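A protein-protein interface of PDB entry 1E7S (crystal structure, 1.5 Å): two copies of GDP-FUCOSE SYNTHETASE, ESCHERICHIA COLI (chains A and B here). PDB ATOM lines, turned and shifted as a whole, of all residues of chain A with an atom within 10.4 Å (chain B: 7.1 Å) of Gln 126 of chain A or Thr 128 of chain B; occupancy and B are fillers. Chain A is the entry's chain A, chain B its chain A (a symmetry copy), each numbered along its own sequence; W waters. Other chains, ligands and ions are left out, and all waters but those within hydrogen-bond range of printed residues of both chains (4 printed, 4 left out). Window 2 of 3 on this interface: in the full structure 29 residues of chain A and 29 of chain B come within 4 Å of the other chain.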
ATOM      1  N   CYS A 109      -8.362 -19.440 -19.793  1.00  0.00           N
ATOM      2  CA  CYS A 109      -8.019 -18.515 -18.691  1.00  0.00           C
ATOM      3  C   CYS A 109      -7.264 -19.249 -17.602  1.00  0.00           C
ATOM      4  O   CYS A 109      -6.759 -18.583 -16.647  1.00  0.00           O
ATOM      5  CB  CYS A 109      -9.342 -17.920 -17.901  1.00  0.00           C
ATOM      6  SG  CYS A 109     -10.104 -16.998 -19.304  1.00  0.00           S
ATOM      7  N   ILE A 110      -7.137 -20.541 -17.661  1.00  0.00           N
ATOM      8  CA  ILE A 110      -6.382 -21.320 -16.694  1.00  0.00           C
ATOM      9  C   ILE A 110      -4.917 -20.935 -16.687  1.00  0.00           C
ATOM     10  O   ILE A 110      -4.238 -21.299 -15.720  1.00  0.00           O
ATOM     11  CB  ILE A 110      -6.528 -22.838 -16.815  1.00  0.00           C
ATOM     12  CG1 ILE A 110      -5.953 -23.402 -18.096  1.00  0.00           C
ATOM     13  CG2 ILE A 110      -7.970 -23.288 -16.583  1.00  0.00           C
ATOM     14  CD1 ILE A 110      -5.924 -24.878 -18.220  1.00  0.00           C
ATOM     15  N   TYR A 111      -4.401 -20.422 -17.811  1.00  0.00           N
ATOM     16  CA  TYR A 111      -2.948 -20.231 -17.918  1.00  0.00           C
ATOM     17  C   TYR A 111      -2.470 -18.920 -17.297  1.00  0.00           C
ATOM     18  O   TYR A 111      -3.202 -17.935 -17.232  1.00  0.00           O
ATOM     19  CB  TYR A 111      -2.557 -20.299 -19.420  1.00  0.00           C
ATOM     20  CG  TYR A 111      -2.662 -21.720 -19.959  1.00  0.00           C
ATOM     21  CD1 TYR A 111      -1.840 -22.725 -19.474  1.00  0.00           C
ATOM     22  CD2 TYR A 111      -3.601 -22.030 -20.916  1.00  0.00           C
ATOM     23  CE1 TYR A 111      -1.966 -24.024 -19.920  1.00  0.00           C
ATOM     24  CE2 TYR A 111      -3.722 -23.331 -21.434  1.00  0.00           C
ATOM     25  CZ  TYR A 111      -2.892 -24.306 -20.920  1.00  0.00           C
ATOM     26  OH  TYR A 111      -3.052 -25.616 -21.323  1.00  0.00           O
ATOM     27  N   PRO A 112      -1.206 -18.928 -16.842  1.00  0.00           N
ATOM     28  CA  PRO A 112      -0.636 -17.724 -16.268  1.00  0.00           C
ATOM     29  C   PRO A 112      -0.680 -16.544 -17.215  1.00  0.00           C
ATOM     30  O   PRO A 112      -0.559 -16.696 -18.437  1.00  0.00           O
ATOM     31  CB  PRO A 112       0.828 -18.104 -15.974  1.00  0.00           C
ATOM     32  CG  PRO A 112       0.736 -19.606 -15.813  1.00  0.00           C
ATOM     33  CD  PRO A 112      -0.275 -20.064 -16.856  1.00  0.00           C
ATOM     34  N   LYS A 113      -0.810 -15.336 -16.682  1.00  0.00           N
ATOM     35  CA  LYS A 113      -0.817 -14.096 -17.475  1.00  0.00           C
ATOM     36  C   LYS A 113       0.444 -13.987 -18.310  1.00  0.00           C
ATOM     37  O   LYS A 113       0.379 -13.609 -19.492  1.00  0.00           O
ATOM     38  CB  LYS A 113      -1.018 -12.830 -16.613  1.00  0.00           C
ATOM     39  CG  LYS A 113      -0.951 -11.537 -17.461  1.00  0.00           C
ATOM     40  N   LEU A 114       1.587 -14.319 -17.723  1.00  0.00           N
ATOM     41  CA  LEU A 114       2.869 -14.215 -18.444  1.00  0.00           C
ATOM     42  C   LEU A 114       3.469 -15.548 -18.851  1.00  0.00           C
ATOM     43  O   LEU A 114       4.695 -15.718 -18.933  1.00  0.00           O
ATOM     44  CB  LEU A 114       3.857 -13.394 -17.599  1.00  0.00           C
ATOM     45  CG  LEU A 114       3.399 -11.937 -17.396  1.00  0.00           C
ATOM     46  CD1 LEU A 114       4.397 -11.195 -16.507  1.00  0.00           C
ATOM     47  CD2 LEU A 114       3.270 -11.164 -18.705  1.00  0.00           C
ATOM     48  N   ALA A 115       2.680 -16.460 -19.328  1.00  0.00           N
ATOM     49  CA  ALA A 115       3.138 -17.764 -19.801  1.00  0.00           C
ATOM     50  C   ALA A 115       4.030 -17.643 -21.030  1.00  0.00           C
ATOM     51  O   ALA A 115       3.820 -16.766 -21.890  1.00  0.00           O
ATOM     52  CB  ALA A 115       1.882 -18.533 -20.202  1.00  0.00           C
ATOM     53  N   LYS A 116       4.880 -18.661 -21.206  1.00  0.00           N
ATOM     54  CA  LYS A 116       5.626 -18.834 -22.456  1.00  0.00           C
ATOM     55  C   LYS A 116       4.714 -19.163 -23.640  1.00  0.00           C
ATOM     56  O   LYS A 116       3.786 -19.928 -23.487  1.00  0.00           O
ATOM     57  CB  LYS A 116       6.646 -19.945 -22.241  1.00  0.00           C
ATOM     58  N   MET A 119       1.435 -21.501 -25.681  1.00  0.00           N
ATOM     59  CA  MET A 119       1.275 -22.081 -24.355  1.00  0.00           C
ATOM     60  C   MET A 119       0.981 -23.574 -24.457  1.00  0.00           C
ATOM     61  O   MET A 119      -0.120 -24.000 -24.788  1.00  0.00           O
ATOM     62  CB  MET A 119       0.170 -21.375 -23.566  1.00  0.00           C
ATOM     63  CG  MET A 119       0.456 -19.857 -23.460  1.00  0.00           C
ATOM     64  SD  MET A 119      -0.760 -18.987 -22.422  1.00  0.00           S
ATOM     65  CE  MET A 119      -2.225 -19.058 -23.411  1.00  0.00           C
ATOM     66  N   ALA A 120       1.964 -24.400 -24.103  1.00  0.00           N
ATOM     67  CA  ALA A 120       1.801 -25.846 -23.962  1.00  0.00           C
ATOM     68  C   ALA A 120       1.019 -26.102 -22.674  1.00  0.00           C
ATOM     69  O   ALA A 120       0.929 -25.254 -21.754  1.00  0.00           O
ATOM     70  CB  ALA A 120       3.175 -26.499 -23.910  1.00  0.00           C
ATOM     71  N   GLU A 121       0.473 -27.314 -22.578  1.00  0.00           N
ATOM     72  CA  GLU A 121      -0.309 -27.676 -21.402  1.00  0.00           C
ATOM     73  C   GLU A 121       0.468 -27.582 -20.096  1.00  0.00           C
ATOM     74  O   GLU A 121      -0.102 -27.202 -19.049  1.00  0.00           O
ATOM     75  CB  GLU A 121      -0.901 -29.064 -21.598  1.00  0.00           C
ATOM     76  CG  GLU A 121      -2.014 -29.180 -22.635  1.00  0.00           C
ATOM     77  CD  GLU A 121      -1.537 -29.347 -24.058  1.00  0.00           C
ATOM     78  OE1 GLU A 121      -0.327 -29.356 -24.363  1.00  0.00           O
ATOM     79  OE2 GLU A 121      -2.437 -29.477 -24.938  1.00  0.00           O
ATOM     80  N   SER A 122       1.766 -27.814 -20.183  1.00  0.00           N
ATOM     81  CA  SER A 122       2.647 -27.700 -19.025  1.00  0.00           C
ATOM     82  C   SER A 122       2.811 -26.264 -18.528  1.00  0.00           C
ATOM     83  O   SER A 122       3.368 -26.149 -17.416  1.00  0.00           O
ATOM     84  CB  SER A 122       4.042 -28.240 -19.362  1.00  0.00           C
ATOM     85  OG  SER A 122       4.526 -27.582 -20.533  1.00  0.00           O
ATOM     86  N   GLU A 123       2.263 -25.258 -19.208  1.00  0.00           N
ATOM     87  CA  GLU A 123       2.277 -23.926 -18.591  1.00  0.00           C
ATOM     88  C   GLU A 123       1.304 -23.771 -17.443  1.00  0.00           C
ATOM     89  O   GLU A 123       1.379 -22.771 -16.700  1.00  0.00           O
ATOM     90  CB  GLU A 123       1.978 -22.858 -19.641  1.00  0.00           C
ATOM     91  CG  GLU A 123       3.068 -22.674 -20.656  1.00  0.00           C
ATOM     92  CD  GLU A 123       4.420 -22.306 -20.112  1.00  0.00           C
ATOM     93  OE1 GLU A 123       4.447 -21.210 -19.489  1.00  0.00           O
ATOM     94  OE2 GLU A 123       5.315 -22.707 -20.889  1.00  0.00           O
ATOM     95  N   LEU A 124       0.364 -24.703 -17.287  1.00  0.00           N
ATOM     96  CA  LEU A 124      -0.599 -24.630 -16.177  1.00  0.00           C
ATOM     97  C   LEU A 124       0.104 -24.559 -14.818  1.00  0.00           C
ATOM     98  O   LEU A 124       1.026 -25.328 -14.548  1.00  0.00           O
ATOM     99  CB  LEU A 124      -1.522 -25.847 -16.208  1.00  0.00           C
ATOM    100  CG  LEU A 124      -2.513 -25.976 -15.068  1.00  0.00           C
ATOM    101  CD1 LEU A 124      -3.465 -24.809 -15.041  1.00  0.00           C
ATOM    102  CD2 LEU A 124      -3.308 -27.286 -15.195  1.00  0.00           C
ATOM    103  N   LEU A 125      -0.313 -23.559 -14.030  1.00  0.00           N
ATOM    104  CA  LEU A 125       0.202 -23.407 -12.674  1.00  0.00           C
ATOM    105  C   LEU A 125       1.621 -22.898 -12.594  1.00  0.00           C
ATOM    106  O   LEU A 125       2.180 -22.865 -11.478  1.00  0.00           O
ATOM    107  CB  LEU A 125      -0.109 -24.602 -11.787  1.00  0.00           C
ATOM    108  CG  LEU A 125      -1.612 -24.800 -11.468  1.00  0.00           C
ATOM    109  CD1 LEU A 125      -1.929 -26.239 -11.068  1.00  0.00           C
ATOM    110  CD2 LEU A 125      -2.138 -23.812 -10.434  1.00  0.00           C
ATOM    111  N   GLN A 126       2.206 -22.434 -13.698  1.00  0.00           N
ATOM    112  CA  GLN A 126       3.577 -21.963 -13.668  1.00  0.00           C
ATOM    113  C   GLN A 126       3.756 -20.529 -13.209  1.00  0.00           C
ATOM    114  O   GLN A 126       4.902 -20.093 -13.086  1.00  0.00           O
ATOM    115  CB  GLN A 126       4.292 -22.163 -15.011  1.00  0.00           C
ATOM    116  CG  GLN A 126       4.320 -23.579 -15.511  1.00  0.00           C
ATOM    117  CD  GLN A 126       5.338 -24.524 -14.964  1.00  0.00           C
ATOM    118  OE1 GLN A 126       5.627 -25.543 -15.673  1.00  0.00           O
ATOM    119  NE2 GLN A 126       6.205 -24.068 -14.105  1.00  0.00           N
ATOM    120  N   GLY A 127       2.694 -19.780 -12.960  1.00  0.00           N
ATOM    121  CA  GLY A 127       2.781 -18.365 -12.599  1.00  0.00           C
ATOM    122  C   GLY A 127       1.417 -17.764 -12.321  1.00  0.00           C
ATOM    123  O   GLY A 127       0.391 -18.434 -12.467  1.00  0.00           O
ATOM    124  N   THR A 128       1.383 -16.520 -11.867  1.00  0.00           N
ATOM    125  CA  THR A 128       0.232 -15.754 -11.482  1.00  0.00           C
ATOM    126  C   THR A 128      -0.810 -15.661 -12.597  1.00  0.00           C
ATOM    127  O   THR A 128      -0.487 -15.516 -13.790  1.00  0.00           O
ATOM    128  CB  THR A 128       0.762 -14.245 -11.213  1.00  0.00           C
ATOM    129  OG1 THR A 128       1.404 -14.488  -9.956  1.00  0.00           O
ATOM    130  CG2 THR A 128      -0.394 -13.326 -10.806  1.00  0.00           C
ATOM    131  N   LEU A 129      -2.078 -15.724 -12.230  1.00  0.00           N
ATOM    132  CA  LEU A 129      -3.232 -15.609 -13.127  1.00  0.00           C
ATOM    133  C   LEU A 129      -3.566 -14.167 -13.460  1.00  0.00           C
ATOM    134  O   LEU A 129      -3.237 -13.282 -12.680  1.00  0.00           O
ATOM    135  CB  LEU A 129      -4.428 -16.325 -12.502  1.00  0.00           C
ATOM    136  CG  LEU A 129      -4.273 -17.830 -12.294  1.00  0.00           C
ATOM    137  CD1 LEU A 129      -5.298 -18.367 -11.319  1.00  0.00           C
ATOM    138  CD2 LEU A 129      -4.367 -18.585 -13.619  1.00  0.00           C
ATOM    139  N   ILE A 138      -9.483 -20.278 -11.180  1.00  0.00           N
ATOM    140  CA  ILE A 138      -9.263 -21.264 -10.097  1.00  0.00           C
ATOM    141  C   ILE A 138     -10.372 -22.315 -10.108  1.00  0.00           C
ATOM    142  O   ILE A 138     -10.061 -23.496  -9.931  1.00  0.00           O
ATOM    143  CB  ILE A 138      -9.079 -20.526  -8.806  1.00  0.00           C
ATOM    144  CG1 ILE A 138      -7.826 -19.638  -8.686  1.00  0.00           C
ATOM    145  CG2 ILE A 138      -9.262 -21.449  -7.639  1.00  0.00           C
ATOM    146  CD1 ILE A 138      -6.593 -20.559  -8.629  1.00  0.00           C
ATOM    147  N   ILE A 141      -9.540 -24.676 -13.015  1.00  0.00           N
ATOM    148  CA  ILE A 141      -8.409 -25.536 -12.659  1.00  0.00           C
ATOM    149  C   ILE A 141      -8.862 -26.618 -11.671  1.00  0.00           C
ATOM    150  O   ILE A 141      -8.486 -27.808 -11.845  1.00  0.00           O
ATOM    151  CB  ILE A 141      -7.279 -24.698 -12.030  1.00  0.00           C
ATOM    152  CG1 ILE A 141      -6.682 -23.797 -13.139  1.00  0.00           C
ATOM    153  CG2 ILE A 141      -6.187 -25.579 -11.458  1.00  0.00           C
ATOM    154  CD1 ILE A 141      -5.732 -22.752 -12.643  1.00  0.00           C
ATOM    155  N   LYS A 145      -8.520 -30.770 -11.897  1.00  0.00           N
ATOM    156  CA  LYS A 145      -7.914 -31.555 -10.830  1.00  0.00           C
ATOM    157  C   LYS A 145      -8.888 -32.527 -10.193  1.00  0.00           C
ATOM    158  O   LYS A 145      -8.481 -33.601  -9.730  1.00  0.00           O
ATOM    159  CB  LYS A 145      -7.178 -30.631  -9.840  1.00  0.00           C
ATOM    160  CG  LYS A 145      -6.086 -29.784 -10.506  1.00  0.00           C
ATOM    161  CD  LYS A 145      -4.982 -30.658 -11.052  1.00  0.00           C
ATOM    162  CE  LYS A 145      -4.015 -29.886 -11.929  1.00  0.00           C
ATOM    163  NZ  LYS A 145      -2.955 -30.800 -12.512  1.00  0.00           N
ATOM    164  N   MET A 239      -1.394 -36.347 -14.081  1.00  0.00           N
ATOM    165  CA  MET A 239      -1.492 -35.076 -13.394  1.00  0.00           C
ATOM    166  C   MET A 239      -1.189 -33.895 -14.281  1.00  0.00           C
ATOM    167  O   MET A 239      -1.055 -32.764 -13.819  1.00  0.00           O
ATOM    168  CB  MET A 239      -0.618 -35.099 -12.158  1.00  0.00           C
ATOM    169  CG  MET A 239      -0.945 -36.167 -11.165  1.00  0.00           C
ATOM    170  SD  MET A 239       0.037 -36.162  -9.642  1.00  0.00           S
ATOM    171  CE  MET A 239      -0.555 -34.683  -8.803  1.00  0.00           C
ATOM    172  N   LEU A 240      -1.208 -34.132 -15.605  1.00  0.00           N
ATOM    173  CA  LEU A 240      -1.108 -33.084 -16.611  1.00  0.00           C
ATOM    174  C   LEU A 240      -1.898 -33.603 -17.806  1.00  0.00           C
ATOM    175  O   LEU A 240      -1.342 -33.894 -18.872  1.00  0.00           O
ATOM    176  CB  LEU A 240       0.313 -32.655 -16.966  1.00  0.00           C
ATOM    177  CG  LEU A 240       0.350 -31.352 -17.804  1.00  0.00           C
ATOM    178  CD1 LEU A 240       0.121 -30.144 -16.929  1.00  0.00           C
ATOM    179  CD2 LEU A 240       1.653 -31.226 -18.563  1.00  0.00           C
ATOM    180  N   HIS A 242      -5.021 -32.451 -19.359  1.00  0.00           N
ATOM    181  CA  HIS A 242      -5.871 -31.657 -20.231  1.00  0.00           C
ATOM    182  C   HIS A 242      -5.227 -31.450 -21.609  1.00  0.00           C
ATOM    183  O   HIS A 242      -4.035 -31.631 -21.792  1.00  0.00           O
ATOM    184  CB  HIS A 242      -6.183 -30.292 -19.585  1.00  0.00           C
ATOM    185  CG  HIS A 242      -4.963 -29.459 -19.321  1.00  0.00           C
ATOM    186  ND1 HIS A 242      -4.614 -28.355 -20.068  1.00  0.00           N
ATOM    187  CD2 HIS A 242      -4.006 -29.666 -18.385  1.00  0.00           C
ATOM    188  CE1 HIS A 242      -3.470 -27.839 -19.570  1.00  0.00           C
ATOM    189  NE2 HIS A 242      -3.115 -28.658 -18.586  1.00  0.00           N
ATOM    190  N   TYR B 111       1.672 -23.405  -1.189  1.00  0.00           N
ATOM    191  CA  TYR B 111       2.795 -22.748  -1.870  1.00  0.00           C
ATOM    192  C   TYR B 111       3.514 -23.665  -2.859  1.00  0.00           C
ATOM    193  O   TYR B 111       3.536 -24.884  -2.705  1.00  0.00           O
ATOM    194  CB  TYR B 111       3.783 -22.225  -0.790  1.00  0.00           C
ATOM    195  CG  TYR B 111       3.209 -21.028  -0.044  1.00  0.00           C
ATOM    196  CD1 TYR B 111       2.956 -19.836  -0.703  1.00  0.00           C
ATOM    197  CD2 TYR B 111       2.904 -21.128   1.295  1.00  0.00           C
ATOM    198  CE1 TYR B 111       2.389 -18.765  -0.045  1.00  0.00           C
ATOM    199  CE2 TYR B 111       2.375 -20.041   2.011  1.00  0.00           C
ATOM    200  CZ  TYR B 111       2.129 -18.874   1.319  1.00  0.00           C
ATOM    201  OH  TYR B 111       1.511 -17.821   1.960  1.00  0.00           O
ATOM    202  N   PRO B 112       4.117 -23.041  -3.884  1.00  0.00           N
ATOM    203  CA  PRO B 112       4.862 -23.813  -4.861  1.00  0.00           C
ATOM    204  C   PRO B 112       5.962 -24.644  -4.238  1.00  0.00           C
ATOM    205  O   PRO B 112       6.582 -24.249  -3.243  1.00  0.00           O
ATOM    206  CB  PRO B 112       5.476 -22.749  -5.792  1.00  0.00           C
ATOM    207  CG  PRO B 112       4.510 -21.595  -5.629  1.00  0.00           C
ATOM    208  CD  PRO B 112       4.120 -21.598  -4.157  1.00  0.00           C
ATOM    209  N   LYS B 113       6.266 -25.796  -4.824  1.00  0.00           N
ATOM    210  CA  LYS B 113       7.345 -26.683  -4.360  1.00  0.00           C
ATOM    211  C   LYS B 113       8.666 -25.940  -4.316  1.00  0.00           C
ATOM    212  O   LYS B 113       9.433 -26.088  -3.348  1.00  0.00           O
ATOM    213  CB  LYS B 113       7.466 -27.975  -5.197  1.00  0.00           C
ATOM    214  CG  LYS B 113       8.651 -28.856  -4.733  1.00  0.00           C
ATOM    215  N   LEU B 114       8.944 -25.141  -5.337  1.00  0.00           N
ATOM    216  CA  LEU B 114      10.220 -24.403  -5.399  1.00  0.00           C
ATOM    217  C   LEU B 114      10.094 -22.913  -5.138  1.00  0.00           C
ATOM    218  O   LEU B 114      10.856 -22.088  -5.665  1.00  0.00           O
ATOM    219  CB  LEU B 114      10.894 -24.676  -6.753  1.00  0.00           C
ATOM    220  CG  LEU B 114      11.285 -26.155  -6.937  1.00  0.00           C
ATOM    221  CD1 LEU B 114      11.901 -26.365  -8.319  1.00  0.00           C
ATOM    222  CD2 LEU B 114      12.290 -26.639  -5.895  1.00  0.00           C
ATOM    223  N   ALA B 115       9.314 -22.518  -4.180  1.00  0.00           N
ATOM    224  CA  ALA B 115       9.145 -21.119  -3.795  1.00  0.00           C
ATOM    225  C   ALA B 115      10.429 -20.523  -3.234  1.00  0.00           C
ATOM    226  O   ALA B 115      11.208 -21.213  -2.548  1.00  0.00           O
ATOM    227  CB  ALA B 115       8.094 -21.110  -2.688  1.00  0.00           C
ATOM    228  N   LEU B 125       0.739 -19.229  -5.936  1.00  0.00           N
ATOM    229  CA  LEU B 125       0.474 -19.299  -7.368  1.00  0.00           C
ATOM    230  C   LEU B 125       1.654 -18.952  -8.244  1.00  0.00           C
ATOM    231  O   LEU B 125       1.475 -18.860  -9.476  1.00  0.00           O
ATOM    232  CB  LEU B 125      -0.840 -18.638  -7.757  1.00  0.00           C
ATOM    233  CG  LEU B 125      -2.107 -19.354  -7.228  1.00  0.00           C
ATOM    234  CD1 LEU B 125      -3.310 -18.415  -7.163  1.00  0.00           C
ATOM    235  CD2 LEU B 125      -2.442 -20.625  -7.998  1.00  0.00           C
ATOM    236  N   GLN B 126       2.859 -18.826  -7.688  1.00  0.00           N
ATOM    237  CA  GLN B 126       4.011 -18.466  -8.491  1.00  0.00           C
ATOM    238  C   GLN B 126       4.682 -19.621  -9.210  1.00  0.00           C
ATOM    239  O   GLN B 126       5.618 -19.370  -9.971  1.00  0.00           O
ATOM    240  CB  GLN B 126       5.059 -17.685  -7.688  1.00  0.00           C
ATOM    241  CG  GLN B 126       4.557 -16.426  -7.042  1.00  0.00           C
ATOM    242  CD  GLN B 126       4.436 -15.185  -7.864  1.00  0.00           C
ATOM    243  OE1 GLN B 126       4.430 -14.073  -7.243  1.00  0.00           O
ATOM    244  NE2 GLN B 126       4.824 -15.228  -9.107  1.00  0.00           N
ATOM    245  N   GLY B 127       4.260 -20.858  -9.005  1.00  0.00           N
ATOM    246  CA  GLY B 127       4.910 -22.031  -9.591  1.00  0.00           C
ATOM    247  C   GLY B 127       4.192 -23.317  -9.232  1.00  0.00           C
ATOM    248  O   GLY B 127       3.218 -23.306  -8.474  1.00  0.00           O
ATOM    249  N   THR B 128       4.620 -24.432  -9.806  1.00  0.00           N
ATOM    250  CA  THR B 128       4.079 -25.754  -9.674  1.00  0.00           C
ATOM    251  C   THR B 128       4.007 -26.215  -8.217  1.00  0.00           C
ATOM    252  O   THR B 128       4.908 -25.956  -7.399  1.00  0.00           O
ATOM    253  CB  THR B 128       5.121 -26.746 -10.424  1.00  0.00           C
ATOM    254  OG1 THR B 128       4.774 -26.406 -11.771  1.00  0.00           O
ATOM    255  CG2 THR B 128       4.650 -28.201 -10.333  1.00  0.00           C
ATOM    256  N   LEU B 129       2.944 -26.919  -7.871  1.00  0.00           N
ATOM    257  CA  LEU B 129       2.699 -27.495  -6.545  1.00  0.00           C
ATOM    258  C   LEU B 129       3.436 -28.804  -6.335  1.00  0.00           C
ATOM    259  O   LEU B 129       3.742 -29.480  -7.310  1.00  0.00           O
ATOM    260  CB  LEU B 129       1.194 -27.669  -6.343  1.00  0.00           C
ATOM    261  CG  LEU B 129       0.367 -26.385  -6.345  1.00  0.00           C
ATOM    262  CD1 LEU B 129      -1.105 -26.670  -6.556  1.00  0.00           C
ATOM    263  CD2 LEU B 129       0.565 -25.595  -5.052  1.00  0.00           C
ATOM    264  N   GLU B 130       3.638 -29.200  -5.079  1.00  0.00           N
ATOM    265  CA  GLU B 130       4.105 -30.569  -4.806  1.00  0.00           C
ATOM    266  C   GLU B 130       3.044 -31.558  -5.258  1.00  0.00           C
ATOM    267  O   GLU B 130       1.888 -31.494  -4.830  1.00  0.00           O
ATOM    268  CB  GLU B 130       4.295 -30.696  -3.288  1.00  0.00           C
ATOM    269  CG  GLU B 130       4.411 -32.139  -2.783  1.00  0.00           C
ATOM    270  CD  GLU B 130       5.525 -32.890  -3.434  1.00  0.00           C
ATOM    271  OE1 GLU B 130       6.663 -32.333  -3.564  1.00  0.00           O
ATOM    272  OE2 GLU B 130       5.228 -34.069  -3.798  1.00  0.00           O
ATOM    273  N   PRO B 131       3.416 -32.565  -6.040  1.00  0.00           N
ATOM    274  CA  PRO B 131       2.411 -33.495  -6.577  1.00  0.00           C
ATOM    275  C   PRO B 131       1.687 -34.298  -5.526  1.00  0.00           C
ATOM    276  O   PRO B 131       0.498 -34.587  -5.685  1.00  0.00           O
ATOM    277  CB  PRO B 131       3.122 -34.312  -7.627  1.00  0.00           C
ATOM    278  CG  PRO B 131       4.565 -34.072  -7.379  1.00  0.00           C
ATOM    279  CD  PRO B 131       4.692 -32.701  -6.774  1.00  0.00           C
ATOM    280  N   GLU B 134      -1.065 -31.935  -4.409  1.00  0.00           N
ATOM    281  CA  GLU B 134      -1.672 -31.044  -5.395  1.00  0.00           C
ATOM    282  C   GLU B 134      -3.188 -30.913  -5.325  1.00  0.00           C
ATOM    283  O   GLU B 134      -3.741 -29.807  -5.280  1.00  0.00           O
ATOM    284  CB  GLU B 134      -1.164 -31.260  -6.821  1.00  0.00           C
ATOM    285  CG  GLU B 134      -1.887 -30.498  -7.903  1.00  0.00           C
ATOM    286  CD  GLU B 134      -1.355 -30.822  -9.289  1.00  0.00           C
ATOM    287  OE1 GLU B 134      -0.355 -30.209  -9.710  1.00  0.00           O
ATOM    288  OE2 GLU B 134      -1.933 -31.649 -10.011  1.00  0.00           O
HETATM  289  O   HOH W   1       6.209 -17.446 -11.954  1.00  0.00           O
HETATM  290  O   HOH W   2       6.920 -23.753 -11.553  1.00  0.00           O
HETATM  291  O   HOH W   3       7.359 -21.013 -12.036  1.00  0.00           O
HETATM  292  O   HOH W   4       4.171 -15.522 -11.678  1.00  0.00           O
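The backbone carbonyl oxygen (O) of Leu 125 of chain B sits at hydrogen-bond distance from the backbone NH (N) of Thr 128 of chain A (3.3 Å). The backbone carbonyl oxygen (O) of Leu 125 of chain A sits at hydrogen-bond distance from the backbone NH (N) of Thr 128 of chain B (3.3 Å). The backbone carbonyl oxygen (O) of Gly 127 of chain A sits close to the backbone carbonyl oxygen (O) of Leu 125 of chain B (3.2 Å). OE2 of Glu 134 of chain B is in salt-bridge range of NZ of Lys 145 of chain A (2.8 Å). The backbone carbonyl oxygen of Gln 126 of chain B sits close to the backbone carbonyl oxygen of Gln 126 of chain A (3.3 Å). O of Leu 125 of chain A sits close to O of Gly 127 of chain B.
O of Thr 128 of chain A lies within hydrogen-bond range of N of Lys 113 of chain A. The backbone carbonyl oxygen of Ser 122 of chain A lies close to the side-chain amide oxygen of Gln 126 of chain A. O of Met 239 of chain A is in hydrogen-bond range of NZ of Lys 145 of chain A (3.0 Å). O of Thr 128 of chain B lies within hydrogen-bond range of N of Lys 113 of chain B (2.9 Å).
Among the printed residues, pairs that only touch across the chains: Gln 126 of chain A with Gly 127 of chain B (3.996 Å), Gln 126 of chain A with Thr 128 of chain B (3.6 Å), Gly 127 of chain A with Gln 126 of chain B (3.996 Å), Thr 128 of chain A with Gln 126 of chain B (3.6 Å), Met 239 of chain A with Pro 131 of chain B (3.3 Å) and Met 239 of chain A with Glu 134 of chain B (3.5 Å).
Of the printed residues of chain B, Gln 126 of chain A touches Gln 126 (3.3 Å), Gly 127 (3.996 Å) and Thr 128 (3.6 Å). Of the printed residues of chain A, Thr 128 of chain B touches Leu 125 and Gln 126. No residue of chain A comes within 4 Å of Pro 112 of chain B. No residue of chain A comes within 4 Å of Leu 129 of chain B. Of the printed residues of chain A, Leu 125 of chain B touches Gly 127 and Thr 128. Printed residues of chain A within 4 Å of Gly 127 of chain B: Leu 125 and Gln 126. Printed residues of chain B within 4 Å of Leu 125 of chain A: Gly 127 and Thr 128. Printed residues of chain B within 4 Å of Thr 128 of chain A: Leu 125 and Gln 126. Lys 113 of chain A touches none of the printed residues of chain B. Tyr 111 of chain A touches none of the printed residues of chain B. The nearest printed residue of chain B that does not touch Gln 126 of chain A is Leu 125 of chain B (4.7 Å). The nearest residue of chain A that does not touch Thr 128 of chain B is Leu 124 of chain A (4.8 Å). The nearest printed residue of chain B that does not touch Lys 145 of chain A is Leu 129 of chain B (6.9 Å).
Hydrophobic or aromatic side chains of chain A within 4 Å of the printed part of chain B: Met 239. Printed residues of chain B that touch a printed residue of chain A: Leu 125, Gln 126, Gly 127, Thr 128, Pro 131 and Glu 134. Hydrophobic or aromatic side chains of chain B within 4 Å of the printed part of chain A: Pro 131.
Leu 125 of chain A touches Gly 127 of chain B, and with the chains exchanged Gly 127 of chain A touches Leu 125 of chain B. Leu 125 of chain A touches Thr 128 of chain B, and with the chains exchanged Thr 128 of chain A touches Leu 125 of chain B. Gln 126 of chain A touches Gly 127 of chain B, and with the chains exchanged Gly 127 of chain A touches Gln 126 of chain B. Gln 126 of chain A touches Thr 128 of chain B, and with the chains exchanged Thr 128 of chain A touches Gln 126 of chain B. Positions printed for both chains: 111, 112, 113, 114, 115, 125, 126, 127, 128 and 129. Of the 12 pairs that touch across the chains among the printed residues, 9 have their exchanged pair printed and touching as well.
Water W2 lies within hydrogen-bond range of the side-chain amide nitrogen (NE2) of Gln 126 of chain A (2.7 Å) and the backbone NH (N) of Thr 128 of chain B (3.0 Å). Water W4 lies within hydrogen-bond range of the side-chain amide nitrogen of Gln 126 of chain B (2.7 Å) and the backbone NH of Thr 128 of chain A (3.0 Å). Water W3 bridges the backbone carbonyl oxygen (O) of Gln 126 of chain A (2.8 Å) and the backbone carbonyl oxygen (O) of Gln 126 of chain B (3.2 Å). Water W1 lies within hydrogen-bond range of O of Gln 126 of chain B (2.8 Å) and O of Gln 126 of chain A (3.2 Å).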
